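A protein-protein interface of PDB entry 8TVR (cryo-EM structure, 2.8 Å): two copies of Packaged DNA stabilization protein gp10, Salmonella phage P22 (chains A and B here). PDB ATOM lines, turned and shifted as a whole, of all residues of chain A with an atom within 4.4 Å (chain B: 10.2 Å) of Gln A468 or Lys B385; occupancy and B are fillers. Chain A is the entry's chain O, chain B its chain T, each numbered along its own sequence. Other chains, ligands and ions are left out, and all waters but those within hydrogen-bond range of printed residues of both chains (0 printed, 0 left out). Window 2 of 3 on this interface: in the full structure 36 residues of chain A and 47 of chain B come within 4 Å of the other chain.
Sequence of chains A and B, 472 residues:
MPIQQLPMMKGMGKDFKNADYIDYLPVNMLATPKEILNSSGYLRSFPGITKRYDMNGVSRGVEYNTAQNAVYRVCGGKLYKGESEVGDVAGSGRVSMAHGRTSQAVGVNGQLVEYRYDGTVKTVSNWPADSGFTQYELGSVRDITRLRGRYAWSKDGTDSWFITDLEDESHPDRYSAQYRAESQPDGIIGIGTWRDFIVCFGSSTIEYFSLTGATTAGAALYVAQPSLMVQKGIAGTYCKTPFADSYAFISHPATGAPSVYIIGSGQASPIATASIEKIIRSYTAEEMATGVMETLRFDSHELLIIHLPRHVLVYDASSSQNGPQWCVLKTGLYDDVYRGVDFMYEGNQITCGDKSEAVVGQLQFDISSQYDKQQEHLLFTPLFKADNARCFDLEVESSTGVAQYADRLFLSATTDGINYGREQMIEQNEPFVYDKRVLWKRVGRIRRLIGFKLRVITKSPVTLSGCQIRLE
The side-chain carboxylate (OE1) of Glu A397 is in salt-bridge range of the guanidinium group (NH1) of Arg B448, 2.7 Å away.
The backbone NH of Ala B386 is in hydrogen-bond range of the backbone carbonyl oxygen of Arg B448, 3.2 Å away. The backbone carbonyl oxygen (O) of Asn A38 is in hydrogen-bond range of the side-chain amide nitrogen (NE2) of Gln A5 (2.6 Å). O of Glu A395 lies within hydrogen-bond range of N of Gln A468 (2.9 Å). The side-chain amino group of Lys B385 is in salt-bridge range of the side-chain carboxylate of Asp B387 (3.1 Å).
Among the printed residues, merely in contact across the chains: Glu A397 with Lys B385, Gln A468 with Lys B385, Leu A37 with Lys B385, Leu A37 with Leu B449, Asn A38 with Lys B385, Leu A37 with Leu B383 and Leu A37 with Phe B384.
Of the printed residues of chain B, Leu A37 touches Leu B383, Phe B384, Lys B385 and Leu B449. Printed residues of chain B within 4 Å of Asn A38: Lys B385. No residue of chain B comes within 4 Å of Leu A394. Of the printed residues of chain B, Glu A397 touches Lys B385 (3.2 Å) and Arg B448 (2.7 Å). No residue of chain B comes within 4 Å of Cys A467. Gln A468 touches one residue of chain B. No residue of chain B comes within 4 Å of Ile A469. Lys B385 touches four residues of chain A. Printed residues of chain A within 4 Å of Arg B448: Glu A397. Of the printed residues of chain A, Leu B449 touches Leu A37 (3.7 Å). The nearest printed residue of chain A that does not touch Lys B385 is Glu A395 (4.5 Å).
Printed residues of chain B that touch a printed residue of chain A: Leu B383, Phe B384, Lys B385, Arg B448 and Leu B449. Of the 13 printed residues of chain A, 4 touch a printed residue of chain B. Among the printed residues, 8 pairs touch across the chains. Among the printed residues, Asp or Glu carboxylates within 4 Å of a Lys or Arg side-chain nitrogen of the other chain: Glu A397 with Arg B448 (2.7 Å).
2 positions are printed for both chains. Of the 8 pairs that touch across the chains among the printed residues, none has its exchanged pair printed and touching as well.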
ATOM      1  N   ILE A   3       4.280  -6.239   3.649  1.00  0.00           N
ATOM      2  CA  ILE A   3       3.518  -7.051   4.590  1.00  0.00           C
ATOM      3  C   ILE A   3       3.318  -8.438   4.000  1.00  0.00           C
ATOM      4  O   ILE A   3       2.889  -8.583   2.849  1.00  0.00           O
ATOM      5  CB  ILE A   3       2.172  -6.390   4.925  1.00  0.00           C
ATOM      6  CG1 ILE A   3       2.381  -4.926   5.318  1.00  0.00           C
ATOM      7  CG2 ILE A   3       1.468  -7.149   6.036  1.00  0.00           C
ATOM      8  CD1 ILE A   3       2.958  -4.740   6.702  1.00  0.00           C
ATOM      9  N   GLN A   4       3.630  -9.461   4.791  1.00  0.00           N
ATOM     10  CA  GLN A   4       3.499 -10.854   4.394  1.00  0.00           C
ATOM     11  C   GLN A   4       2.546 -11.559   5.348  1.00  0.00           C
ATOM     12  O   GLN A   4       2.666 -11.417   6.570  1.00  0.00           O
ATOM     13  CB  GLN A   4       4.862 -11.552   4.391  1.00  0.00           C
ATOM     14  CG  GLN A   4       4.806 -13.031   4.054  1.00  0.00           C
ATOM     15  CD  GLN A   4       4.548 -13.282   2.584  1.00  0.00           C
ATOM     16  OE1 GLN A   4       5.409 -13.037   1.740  1.00  0.00           O
ATOM     17  NE2 GLN A   4       3.355 -13.774   2.267  1.00  0.00           N
ATOM     18  N   GLN A   5       1.606 -12.316   4.788  1.00  0.00           N
ATOM     19  CA  GLN A   5       0.645 -13.061   5.588  1.00  0.00           C
ATOM     20  C   GLN A   5       1.196 -14.442   5.918  1.00  0.00           C
ATOM     21  O   GLN A   5       1.737 -15.128   5.046  1.00  0.00           O
ATOM     22  CB  GLN A   5      -0.682 -13.190   4.841  1.00  0.00           C
ATOM     23  CG  GLN A   5      -1.342 -11.866   4.512  1.00  0.00           C
ATOM     24  CD  GLN A   5      -2.752 -11.774   5.054  1.00  0.00           C
ATOM     25  OE1 GLN A   5      -2.960 -11.691   6.263  1.00  0.00           O
ATOM     26  NE2 GLN A   5      -3.732 -11.789   4.157  1.00  0.00           N
ATOM     27  N   LEU A  37     -11.600 -10.593   7.137  1.00  0.00           N
ATOM     28  CA  LEU A  37     -11.000  -9.404   6.549  1.00  0.00           C
ATOM     29  C   LEU A  37      -9.551  -9.705   6.184  1.00  0.00           C
ATOM     30  O   LEU A  37      -8.727  -9.973   7.064  1.00  0.00           O
ATOM     31  CB  LEU A  37     -11.118  -8.207   7.502  1.00  0.00           C
ATOM     32  CG  LEU A  37     -10.680  -8.328   8.964  1.00  0.00           C
ATOM     33  CD1 LEU A  37      -9.275  -7.792   9.189  1.00  0.00           C
ATOM     34  CD2 LEU A  37     -11.677  -7.616   9.862  1.00  0.00           C
ATOM     35  N   ASN A  38      -9.241  -9.694   4.889  1.00  0.00           N
ATOM     36  CA  ASN A  38      -7.909 -10.014   4.375  1.00  0.00           C
ATOM     37  C   ASN A  38      -7.419 -11.387   4.831  1.00  0.00           C
ATOM     38  O   ASN A  38      -6.215 -11.661   4.786  1.00  0.00           O
ATOM     39  CB  ASN A  38      -6.886  -8.942   4.775  1.00  0.00           C
ATOM     40  CG  ASN A  38      -7.405  -7.532   4.576  1.00  0.00           C
ATOM     41  OD1 ASN A  38      -8.184  -7.268   3.661  1.00  0.00           O
ATOM     42  ND2 ASN A  38      -6.972  -6.617   5.434  1.00  0.00           N
ATOM     43  N   ASP A 393       6.635  -5.898  13.221  1.00  0.00           N
ATOM     44  CA  ASP A 393       5.178  -5.758  13.282  1.00  0.00           C
ATOM     45  C   ASP A 393       4.458  -7.098  13.128  1.00  0.00           C
ATOM     46  O   ASP A 393       3.751  -7.348  12.150  1.00  0.00           O
ATOM     47  CB  ASP A 393       4.692  -4.760  12.229  1.00  0.00           C
ATOM     48  CG  ASP A 393       5.045  -3.331  12.573  1.00  0.00           C
ATOM     49  OD1 ASP A 393       5.029  -2.989  13.772  1.00  0.00           O
ATOM     50  OD2 ASP A 393       5.343  -2.551  11.646  1.00  0.00           O
ATOM     51  N   LEU A 394       4.646  -7.966  14.118  1.00  0.00           N
ATOM     52  CA  LEU A 394       3.908  -9.226  14.174  1.00  0.00           C
ATOM     53  C   LEU A 394       2.495  -8.923  14.657  1.00  0.00           C
ATOM     54  O   LEU A 394       2.270  -8.669  15.841  1.00  0.00           O
ATOM     55  CB  LEU A 394       4.610 -10.226  15.085  1.00  0.00           C
ATOM     56  CG  LEU A 394       4.557 -11.693  14.653  1.00  0.00           C
ATOM     57  CD1 LEU A 394       5.710 -12.465  15.262  1.00  0.00           C
ATOM     58  CD2 LEU A 394       3.228 -12.327  15.033  1.00  0.00           C
ATOM     59  N   GLU A 395       1.539  -8.946  13.732  1.00  0.00           N
ATOM     60  CA  GLU A 395       0.144  -8.639  14.014  1.00  0.00           C
ATOM     61  C   GLU A 395      -0.709  -9.890  13.871  1.00  0.00           C
ATOM     62  O   GLU A 395      -0.472 -10.718  12.986  1.00  0.00           O
ATOM     63  CB  GLU A 395      -0.384  -7.557  13.066  1.00  0.00           C
ATOM     64  CG  GLU A 395      -0.457  -6.157  13.648  1.00  0.00           C
ATOM     65  CD  GLU A 395      -1.778  -5.876  14.343  1.00  0.00           C
ATOM     66  OE1 GLU A 395      -2.399  -6.827  14.857  1.00  0.00           O
ATOM     67  OE2 GLU A 395      -2.199  -4.702  14.368  1.00  0.00           O
ATOM     68  N   GLU A 397      -5.119 -10.949  14.350  1.00  0.00           N
ATOM     69  CA  GLU A 397      -6.477 -10.486  14.598  1.00  0.00           C
ATOM     70  C   GLU A 397      -7.158 -11.455  15.554  1.00  0.00           C
ATOM     71  O   GLU A 397      -7.249 -12.653  15.269  1.00  0.00           O
ATOM     72  CB  GLU A 397      -7.265 -10.368  13.295  1.00  0.00           C
ATOM     73  CG  GLU A 397      -6.840  -9.201  12.422  1.00  0.00           C
ATOM     74  CD  GLU A 397      -7.310  -7.866  12.964  1.00  0.00           C
ATOM     75  OE1 GLU A 397      -8.229  -7.855  13.811  1.00  0.00           O
ATOM     76  OE2 GLU A 397      -6.759  -6.826  12.548  1.00  0.00           O
ATOM     77  N   GLY A 466      -5.565 -13.889  10.565  1.00  0.00           N
ATOM     78  CA  GLY A 466      -4.835 -12.812   9.927  1.00  0.00           C
ATOM     79  C   GLY A 466      -3.457 -12.526  10.483  1.00  0.00           C
ATOM     80  O   GLY A 466      -3.109 -11.363  10.712  1.00  0.00           O
ATOM     81  N   CYS A 467      -2.661 -13.568  10.707  1.00  0.00           N
ATOM     82  CA  CYS A 467      -1.282 -13.370  11.132  1.00  0.00           C
ATOM     83  C   CYS A 467      -0.481 -12.729  10.007  1.00  0.00           C
ATOM     84  O   CYS A 467      -0.528 -13.183   8.860  1.00  0.00           O
ATOM     85  CB  CYS A 467      -0.655 -14.702  11.540  1.00  0.00           C
ATOM     86  SG  CYS A 467       0.910 -14.555  12.429  1.00  0.00           S
ATOM     87  N   GLN A 468       0.254 -11.669  10.334  1.00  0.00           N
ATOM     88  CA  GLN A 468       1.001 -10.932   9.328  1.00  0.00           C
ATOM     89  C   GLN A 468       2.252 -10.337   9.954  1.00  0.00           C
ATOM     90  O   GLN A 468       2.301 -10.079  11.159  1.00  0.00           O
ATOM     91  CB  GLN A 468       0.146  -9.827   8.700  1.00  0.00           C
ATOM     92  CG  GLN A 468      -0.282  -8.753   9.678  1.00  0.00           C
ATOM     93  CD  GLN A 468      -0.862  -7.538   8.991  1.00  0.00           C
ATOM     94  OE1 GLN A 468      -1.249  -7.596   7.825  1.00  0.00           O
ATOM     95  NE2 GLN A 468      -0.925  -6.426   9.710  1.00  0.00           N
ATOM     96  N   ILE A 469       3.264 -10.124   9.116  1.00  0.00           N
ATOM     97  CA  ILE A 469       4.522  -9.520   9.532  1.00  0.00           C
ATOM     98  C   ILE A 469       4.922  -8.473   8.503  1.00  0.00           C
ATOM     99  O   ILE A 469       4.448  -8.472   7.367  1.00  0.00           O
ATOM    100  CB  ILE A 469       5.649 -10.560   9.697  1.00  0.00           C
ATOM    101  CG1 ILE A 469       5.665 -11.518   8.504  1.00  0.00           C
ATOM    102  CG2 ILE A 469       5.494 -11.318  11.003  1.00  0.00           C
ATOM    103  CD1 ILE A 469       6.861 -12.436   8.473  1.00  0.00           C
ATOM    104  N   GLN B   4     -14.255   2.511  -3.699  1.00  0.00           N
ATOM    105  CA  GLN B   4     -14.379   1.107  -3.334  1.00  0.00           C
ATOM    106  C   GLN B   4     -15.852   0.761  -3.183  1.00  0.00           C
ATOM    107  O   GLN B   4     -16.602   1.492  -2.525  1.00  0.00           O
ATOM    108  CB  GLN B   4     -13.623   0.810  -2.036  1.00  0.00           C
ATOM    109  CG  GLN B   4     -13.828  -0.595  -1.499  1.00  0.00           C
ATOM    110  CD  GLN B   4     -13.089  -1.642  -2.306  1.00  0.00           C
ATOM    111  OE1 GLN B   4     -11.859  -1.692  -2.299  1.00  0.00           O
ATOM    112  NE2 GLN B   4     -13.836  -2.486  -3.005  1.00  0.00           N
ATOM    113  N   LEU B   6     -18.945  -1.451  -1.793  1.00  0.00           N
ATOM    114  CA  LEU B   6     -19.245  -2.182  -0.569  1.00  0.00           C
ATOM    115  C   LEU B   6     -20.449  -3.084  -0.784  1.00  0.00           C
ATOM    116  O   LEU B   6     -21.551  -2.578  -1.042  1.00  0.00           O
ATOM    117  CB  LEU B   6     -19.509  -1.218   0.583  1.00  0.00           C
ATOM    118  CG  LEU B   6     -18.376  -0.272   0.973  1.00  0.00           C
ATOM    119  CD1 LEU B   6     -18.894   0.796   1.918  1.00  0.00           C
ATOM    120  CD2 LEU B   6     -17.234  -1.044   1.606  1.00  0.00           C
ATOM    121  N   MET B  12     -21.579  -8.740   8.087  1.00  0.00           N
ATOM    122  CA  MET B  12     -20.615  -9.499   8.868  1.00  0.00           C
ATOM    123  C   MET B  12     -20.366  -8.789  10.190  1.00  0.00           C
ATOM    124  O   MET B  12     -20.301  -7.558  10.236  1.00  0.00           O
ATOM    125  CB  MET B  12     -19.308  -9.671   8.088  1.00  0.00           C
ATOM    126  CG  MET B  12     -18.121 -10.038   8.937  1.00  0.00           C
ATOM    127  SD  MET B  12     -17.837 -11.810   8.945  1.00  0.00           S
ATOM    128  CE  MET B  12     -16.726 -11.908  10.332  1.00  0.00           C
ATOM    129  N   TYR B  21     -17.459 -15.048  15.039  1.00  0.00           N
ATOM    130  CA  TYR B  21     -17.792 -14.316  13.827  1.00  0.00           C
ATOM    131  C   TYR B  21     -19.078 -14.869  13.226  1.00  0.00           C
ATOM    132  O   TYR B  21     -19.201 -16.079  13.017  1.00  0.00           O
ATOM    133  CB  TYR B  21     -16.651 -14.406  12.814  1.00  0.00           C
ATOM    134  CG  TYR B  21     -15.390 -13.687  13.239  1.00  0.00           C
ATOM    135  CD1 TYR B  21     -15.403 -12.326  13.514  1.00  0.00           C
ATOM    136  CD2 TYR B  21     -14.186 -14.365  13.348  1.00  0.00           C
ATOM    137  CE1 TYR B  21     -14.255 -11.665  13.894  1.00  0.00           C
ATOM    138  CE2 TYR B  21     -13.032 -13.713  13.729  1.00  0.00           C
ATOM    139  CZ  TYR B  21     -13.071 -12.363  14.000  1.00  0.00           C
ATOM    140  OH  TYR B  21     -11.921 -11.708  14.380  1.00  0.00           O
ATOM    141  N   PRO B 382     -19.934  -5.982   5.211  1.00  0.00           N
ATOM    142  CA  PRO B 382     -18.920  -6.751   5.938  1.00  0.00           C
ATOM    143  C   PRO B 382     -17.855  -5.851   6.546  1.00  0.00           C
ATOM    144  O   PRO B 382     -17.578  -4.754   6.057  1.00  0.00           O
ATOM    145  CB  PRO B 382     -18.324  -7.667   4.863  1.00  0.00           C
ATOM    146  CG  PRO B 382     -18.656  -7.016   3.568  1.00  0.00           C
ATOM    147  CD  PRO B 382     -19.939  -6.281   3.770  1.00  0.00           C
ATOM    148  N   LEU B 383     -17.264  -6.329   7.638  1.00  0.00           N
ATOM    149  CA  LEU B 383     -16.155  -5.626   8.266  1.00  0.00           C
ATOM    150  C   LEU B 383     -14.896  -5.738   7.411  1.00  0.00           C
ATOM    151  O   LEU B 383     -14.658  -6.749   6.746  1.00  0.00           O
ATOM    152  CB  LEU B 383     -15.878  -6.194   9.658  1.00  0.00           C
ATOM    153  CG  LEU B 383     -16.775  -5.767  10.818  1.00  0.00           C
ATOM    154  CD1 LEU B 383     -16.879  -6.891  11.835  1.00  0.00           C
ATOM    155  CD2 LEU B 383     -16.241  -4.504  11.473  1.00  0.00           C
ATOM    156  N   PHE B 384     -14.081  -4.686   7.439  1.00  0.00           N
ATOM    157  CA  PHE B 384     -12.814  -4.707   6.722  1.00  0.00           C
ATOM    158  C   PHE B 384     -11.799  -3.846   7.460  1.00  0.00           C
ATOM    159  O   PHE B 384     -12.153  -2.955   8.235  1.00  0.00           O
ATOM    160  CB  PHE B 384     -12.963  -4.244   5.263  1.00  0.00           C
ATOM    161  CG  PHE B 384     -13.790  -3.000   5.090  1.00  0.00           C
ATOM    162  CD1 PHE B 384     -15.172  -3.061   5.088  1.00  0.00           C
ATOM    163  CD2 PHE B 384     -13.181  -1.773   4.902  1.00  0.00           C
ATOM    164  CE1 PHE B 384     -15.933  -1.923   4.921  1.00  0.00           C
ATOM    165  CE2 PHE B 384     -13.936  -0.629   4.731  1.00  0.00           C
ATOM    166  CZ  PHE B 384     -15.315  -0.707   4.738  1.00  0.00           C
ATOM    167  N   LYS B 385     -10.524  -4.133   7.207  1.00  0.00           N
ATOM    168  CA  LYS B 385      -9.410  -3.457   7.856  1.00  0.00           C
ATOM    169  C   LYS B 385      -8.912  -2.337   6.950  1.00  0.00           C
ATOM    170  O   LYS B 385      -8.408  -2.598   5.852  1.00  0.00           O
ATOM    171  CB  LYS B 385      -8.286  -4.445   8.165  1.00  0.00           C
ATOM    172  CG  LYS B 385      -7.316  -3.984   9.238  1.00  0.00           C
ATOM    173  CD  LYS B 385      -6.250  -5.036   9.497  1.00  0.00           C
ATOM    174  CE  LYS B 385      -5.329  -4.624  10.633  1.00  0.00           C
ATOM    175  NZ  LYS B 385      -3.904  -4.573  10.206  1.00  0.00           N
ATOM    176  N   ALA B 386      -9.065  -1.098   7.407  1.00  0.00           N
ATOM    177  CA  ALA B 386      -8.716   0.091   6.635  1.00  0.00           C
ATOM    178  C   ALA B 386      -7.967   1.087   7.515  1.00  0.00           C
ATOM    179  O   ALA B 386      -8.335   2.258   7.611  1.00  0.00           O
ATOM    180  CB  ALA B 386      -9.961   0.726   6.020  1.00  0.00           C
ATOM    181  N   ASP B 387      -6.933   0.613   8.209  1.00  0.00           N
ATOM    182  CA  ASP B 387      -6.202   1.436   9.169  1.00  0.00           C
ATOM    183  C   ASP B 387      -5.781   2.768   8.562  1.00  0.00           C
ATOM    184  O   ASP B 387      -5.083   2.805   7.545  1.00  0.00           O
ATOM    185  CB  ASP B 387      -4.966   0.682   9.668  1.00  0.00           C
ATOM    186  CG  ASP B 387      -5.303  -0.672  10.249  1.00  0.00           C
ATOM    187  OD1 ASP B 387      -6.478  -0.899  10.590  1.00  0.00           O
ATOM    188  OD2 ASP B 387      -4.388  -1.510  10.377  1.00  0.00           O
ATOM    189  N   ASN B 388      -6.214   3.862   9.198  1.00  0.00           N
ATOM    190  CA  ASN B 388      -5.872   5.225   8.783  1.00  0.00           C
ATOM    191  C   ASN B 388      -6.338   5.507   7.354  1.00  0.00           C
ATOM    192  O   ASN B 388      -5.549   5.872   6.480  1.00  0.00           O
ATOM    193  CB  ASN B 388      -4.369   5.487   8.925  1.00  0.00           C
ATOM    194  CG  ASN B 388      -3.842   5.143  10.303  1.00  0.00           C
ATOM    195  OD1 ASN B 388      -4.499   5.387  11.314  1.00  0.00           O
ATOM    196  ND2 ASN B 388      -2.643   4.578  10.350  1.00  0.00           N
ATOM    197  N   ALA B 389      -7.640   5.346   7.118  1.00  0.00           N
ATOM    198  CA  ALA B 389      -8.194   5.498   5.778  1.00  0.00           C
ATOM    199  C   ALA B 389      -8.833   6.858   5.532  1.00  0.00           C
ATOM    200  O   ALA B 389      -8.582   7.462   4.485  1.00  0.00           O
ATOM    201  CB  ALA B 389      -9.223   4.401   5.497  1.00  0.00           C
ATOM    202  N   ARG B 390      -9.651   7.358   6.463  1.00  0.00           N
ATOM    203  CA  ARG B 390     -10.333   8.646   6.311  1.00  0.00           C
ATOM    204  C   ARG B 390     -11.210   8.645   5.052  1.00  0.00           C
ATOM    205  O   ARG B 390     -10.931   9.298   4.047  1.00  0.00           O
ATOM    206  CB  ARG B 390      -9.318   9.800   6.317  1.00  0.00           C
ATOM    207  CG  ARG B 390      -9.914  11.194   6.164  1.00  0.00           C
ATOM    208  CD  ARG B 390     -10.591  11.695   7.430  1.00  0.00           C
ATOM    209  NE  ARG B 390     -10.791  13.140   7.381  1.00  0.00           N
ATOM    210  CZ  ARG B 390     -10.696  13.952   8.424  1.00  0.00           C
ATOM    211  NH1 ARG B 390     -10.446  13.493   9.640  1.00  0.00           N
ATOM    212  NH2 ARG B 390     -10.858  15.259   8.243  1.00  0.00           N
ATOM    213  N   THR B 414     -19.973   0.964  12.695  1.00  0.00           N
ATOM    214  CA  THR B 414     -19.406   0.220  13.809  1.00  0.00           C
ATOM    215  C   THR B 414     -17.906   0.060  13.592  1.00  0.00           C
ATOM    216  O   THR B 414     -17.448  -0.123  12.461  1.00  0.00           O
ATOM    217  CB  THR B 414     -20.083  -1.151  13.968  1.00  0.00           C
ATOM    218  OG1 THR B 414     -19.661  -1.761  15.194  1.00  0.00           O
ATOM    219  CG2 THR B 414     -19.765  -2.077  12.804  1.00  0.00           C
ATOM    220  N   THR B 415     -17.141   0.170  14.675  1.00  0.00           N
ATOM    221  CA  THR B 415     -15.696   0.012  14.621  1.00  0.00           C
ATOM    222  C   THR B 415     -15.208  -1.212  15.383  1.00  0.00           C
ATOM    223  O   THR B 415     -14.001  -1.467  15.410  1.00  0.00           O
ATOM    224  CB  THR B 415     -15.001   1.267  15.161  1.00  0.00           C
ATOM    225  OG1 THR B 415     -15.097   1.294  16.590  1.00  0.00           O
ATOM    226  CG2 THR B 415     -15.643   2.520  14.590  1.00  0.00           C
ATOM    227  N   ILE B 446     -11.049   5.946   9.703  1.00  0.00           N
ATOM    228  CA  ILE B 446     -11.124   4.556  10.134  1.00  0.00           C
ATOM    229  C   ILE B 446      -9.856   4.233  10.908  1.00  0.00           C
ATOM    230  O   ILE B 446      -8.748   4.318  10.367  1.00  0.00           O
ATOM    231  CB  ILE B 446     -11.304   3.608   8.938  1.00  0.00           C
ATOM    232  CG1 ILE B 446     -12.469   4.079   8.066  1.00  0.00           C
ATOM    233  CG2 ILE B 446     -11.516   2.181   9.414  1.00  0.00           C
ATOM    234  CD1 ILE B 446     -12.467   3.505   6.673  1.00  0.00           C
ATOM    235  N   ARG B 447     -10.014   3.869  12.182  1.00  0.00           N
ATOM    236  CA  ARG B 447      -8.857   3.538  13.004  1.00  0.00           C
ATOM    237  C   ARG B 447      -8.347   2.135  12.693  1.00  0.00           C
ATOM    238  O   ARG B 447      -7.219   1.966  12.217  1.00  0.00           O
ATOM    239  CB  ARG B 447      -9.213   3.672  14.486  1.00  0.00           C
ATOM    240  CG  ARG B 447      -8.135   3.174  15.431  1.00  0.00           C
ATOM    241  CD  ARG B 447      -8.134   3.966  16.721  1.00  0.00           C
ATOM    242  NE  ARG B 447      -9.252   3.596  17.581  1.00  0.00           N
ATOM    243  CZ  ARG B 447      -9.315   3.854  18.880  1.00  0.00           C
ATOM    244  NH1 ARG B 447      -8.335   4.481  19.509  1.00  0.00           N
ATOM    245  NH2 ARG B 447     -10.390   3.474  19.564  1.00  0.00           N
ATOM    246  N   ARG B 448      -9.156   1.113  12.972  1.00  0.00           N
ATOM    247  CA  ARG B 448      -8.819  -0.253  12.585  1.00  0.00           C
ATOM    248  C   ARG B 448      -9.850  -0.858  11.642  1.00  0.00           C
ATOM    249  O   ARG B 448      -9.490  -1.299  10.546  1.00  0.00           O
ATOM    250  CB  ARG B 448      -8.656  -1.131  13.833  1.00  0.00           C
ATOM    251  CG  ARG B 448      -7.835  -2.385  13.594  1.00  0.00           C
ATOM    252  CD  ARG B 448      -7.484  -3.081  14.895  1.00  0.00           C
ATOM    253  NE  ARG B 448      -8.667  -3.359  15.700  1.00  0.00           N
ATOM    254  CZ  ARG B 448      -9.171  -4.571  15.890  1.00  0.00           C
ATOM    255  NH1 ARG B 448      -8.612  -5.644  15.357  1.00  0.00           N
ATOM    256  NH2 ARG B 448     -10.266  -4.707  16.630  1.00  0.00           N
ATOM    257  N   LEU B 449     -11.125  -0.877  12.025  1.00  0.00           N
ATOM    258  CA  LEU B 449     -12.173  -1.541  11.264  1.00  0.00           C
ATOM    259  C   LEU B 449     -13.392  -0.634  11.184  1.00  0.00           C
ATOM    260  O   LEU B 449     -13.545   0.305  11.968  1.00  0.00           O
ATOM    261  CB  LEU B 449     -12.568  -2.886  11.890  1.00  0.00           C
ATOM    262  CG  LEU B 449     -11.458  -3.780  12.444  1.00  0.00           C
ATOM    263  CD1 LEU B 449     -12.044  -4.868  13.326  1.00  0.00           C
ATOM    264  CD2 LEU B 449     -10.625  -4.384  11.325  1.00  0.00           C
ATOM    265  N   ILE B 450     -14.265  -0.924  10.219  1.00  0.00           N
ATOM    266  CA  ILE B 450     -15.474  -0.135  10.028  1.00  0.00           C
ATOM    267  C   ILE B 450     -16.507  -0.999   9.322  1.00  0.00           C
ATOM    268  O   ILE B 450     -16.166  -1.937   8.598  1.00  0.00           O
ATOM    269  CB  ILE B 450     -15.173   1.171   9.246  1.00  0.00           C
ATOM    270  CG1 ILE B 450     -16.273   2.206   9.486  1.00  0.00           C
ATOM    271  CG2 ILE B 450     -15.005   0.894   7.769  1.00  0.00           C
ATOM    272  CD1 ILE B 450     -16.360   2.668  10.917  1.00  0.00           C
ATOM    273  N   GLY B 451     -17.780  -0.690   9.558  1.00  0.00           N
ATOM    274  CA  GLY B 451     -18.895  -1.358   8.916  1.00  0.00           C
ATOM    275  C   GLY B 451     -20.167  -0.565   9.128  1.00  0.00           C
ATOM    276  O   GLY B 451     -20.309   0.099  10.156  1.00  0.00           O
ATOM    277  N   ILE B 469     -17.711   3.958  -1.443  1.00  0.00           N
ATOM    278  CA  ILE B 469     -17.046   4.961  -0.625  1.00  0.00           C
ATOM    279  C   ILE B 469     -15.797   5.432  -1.357  1.00  0.00           C
ATOM    280  O   ILE B 469     -15.311   4.784  -2.283  1.00  0.00           O
ATOM    281  CB  ILE B 469     -16.671   4.426   0.773  1.00  0.00           C
ATOM    282  CG1 ILE B 469     -16.039   3.039   0.656  1.00  0.00           C
ATOM    283  CG2 ILE B 469     -17.889   4.397   1.680  1.00  0.00           C
ATOM    284  CD1 ILE B 469     -15.400   2.548   1.930  1.00  0.00           C
ATOM    285  N   LEU B 471     -11.921   6.324  -0.380  1.00  0.00           N
ATOM    286  CA  LEU B 471     -10.989   6.080   0.711  1.00  0.00           C
ATOM    287  C   LEU B 471      -9.829   7.064   0.757  1.00  0.00           C
ATOM    288  O   LEU B 471      -9.055   7.030   1.720  1.00  0.00           O
ATOM    289  CB  LEU B 471     -10.440   4.651   0.625  1.00  0.00           C
ATOM    290  CG  LEU B 471     -11.370   3.547   1.133  1.00  0.00           C
ATOM    291  CD1 LEU B 471     -10.664   2.202   1.118  1.00  0.00           C
ATOM    292  CD2 LEU B 471     -11.891   3.868   2.525  1.00  0.00           C
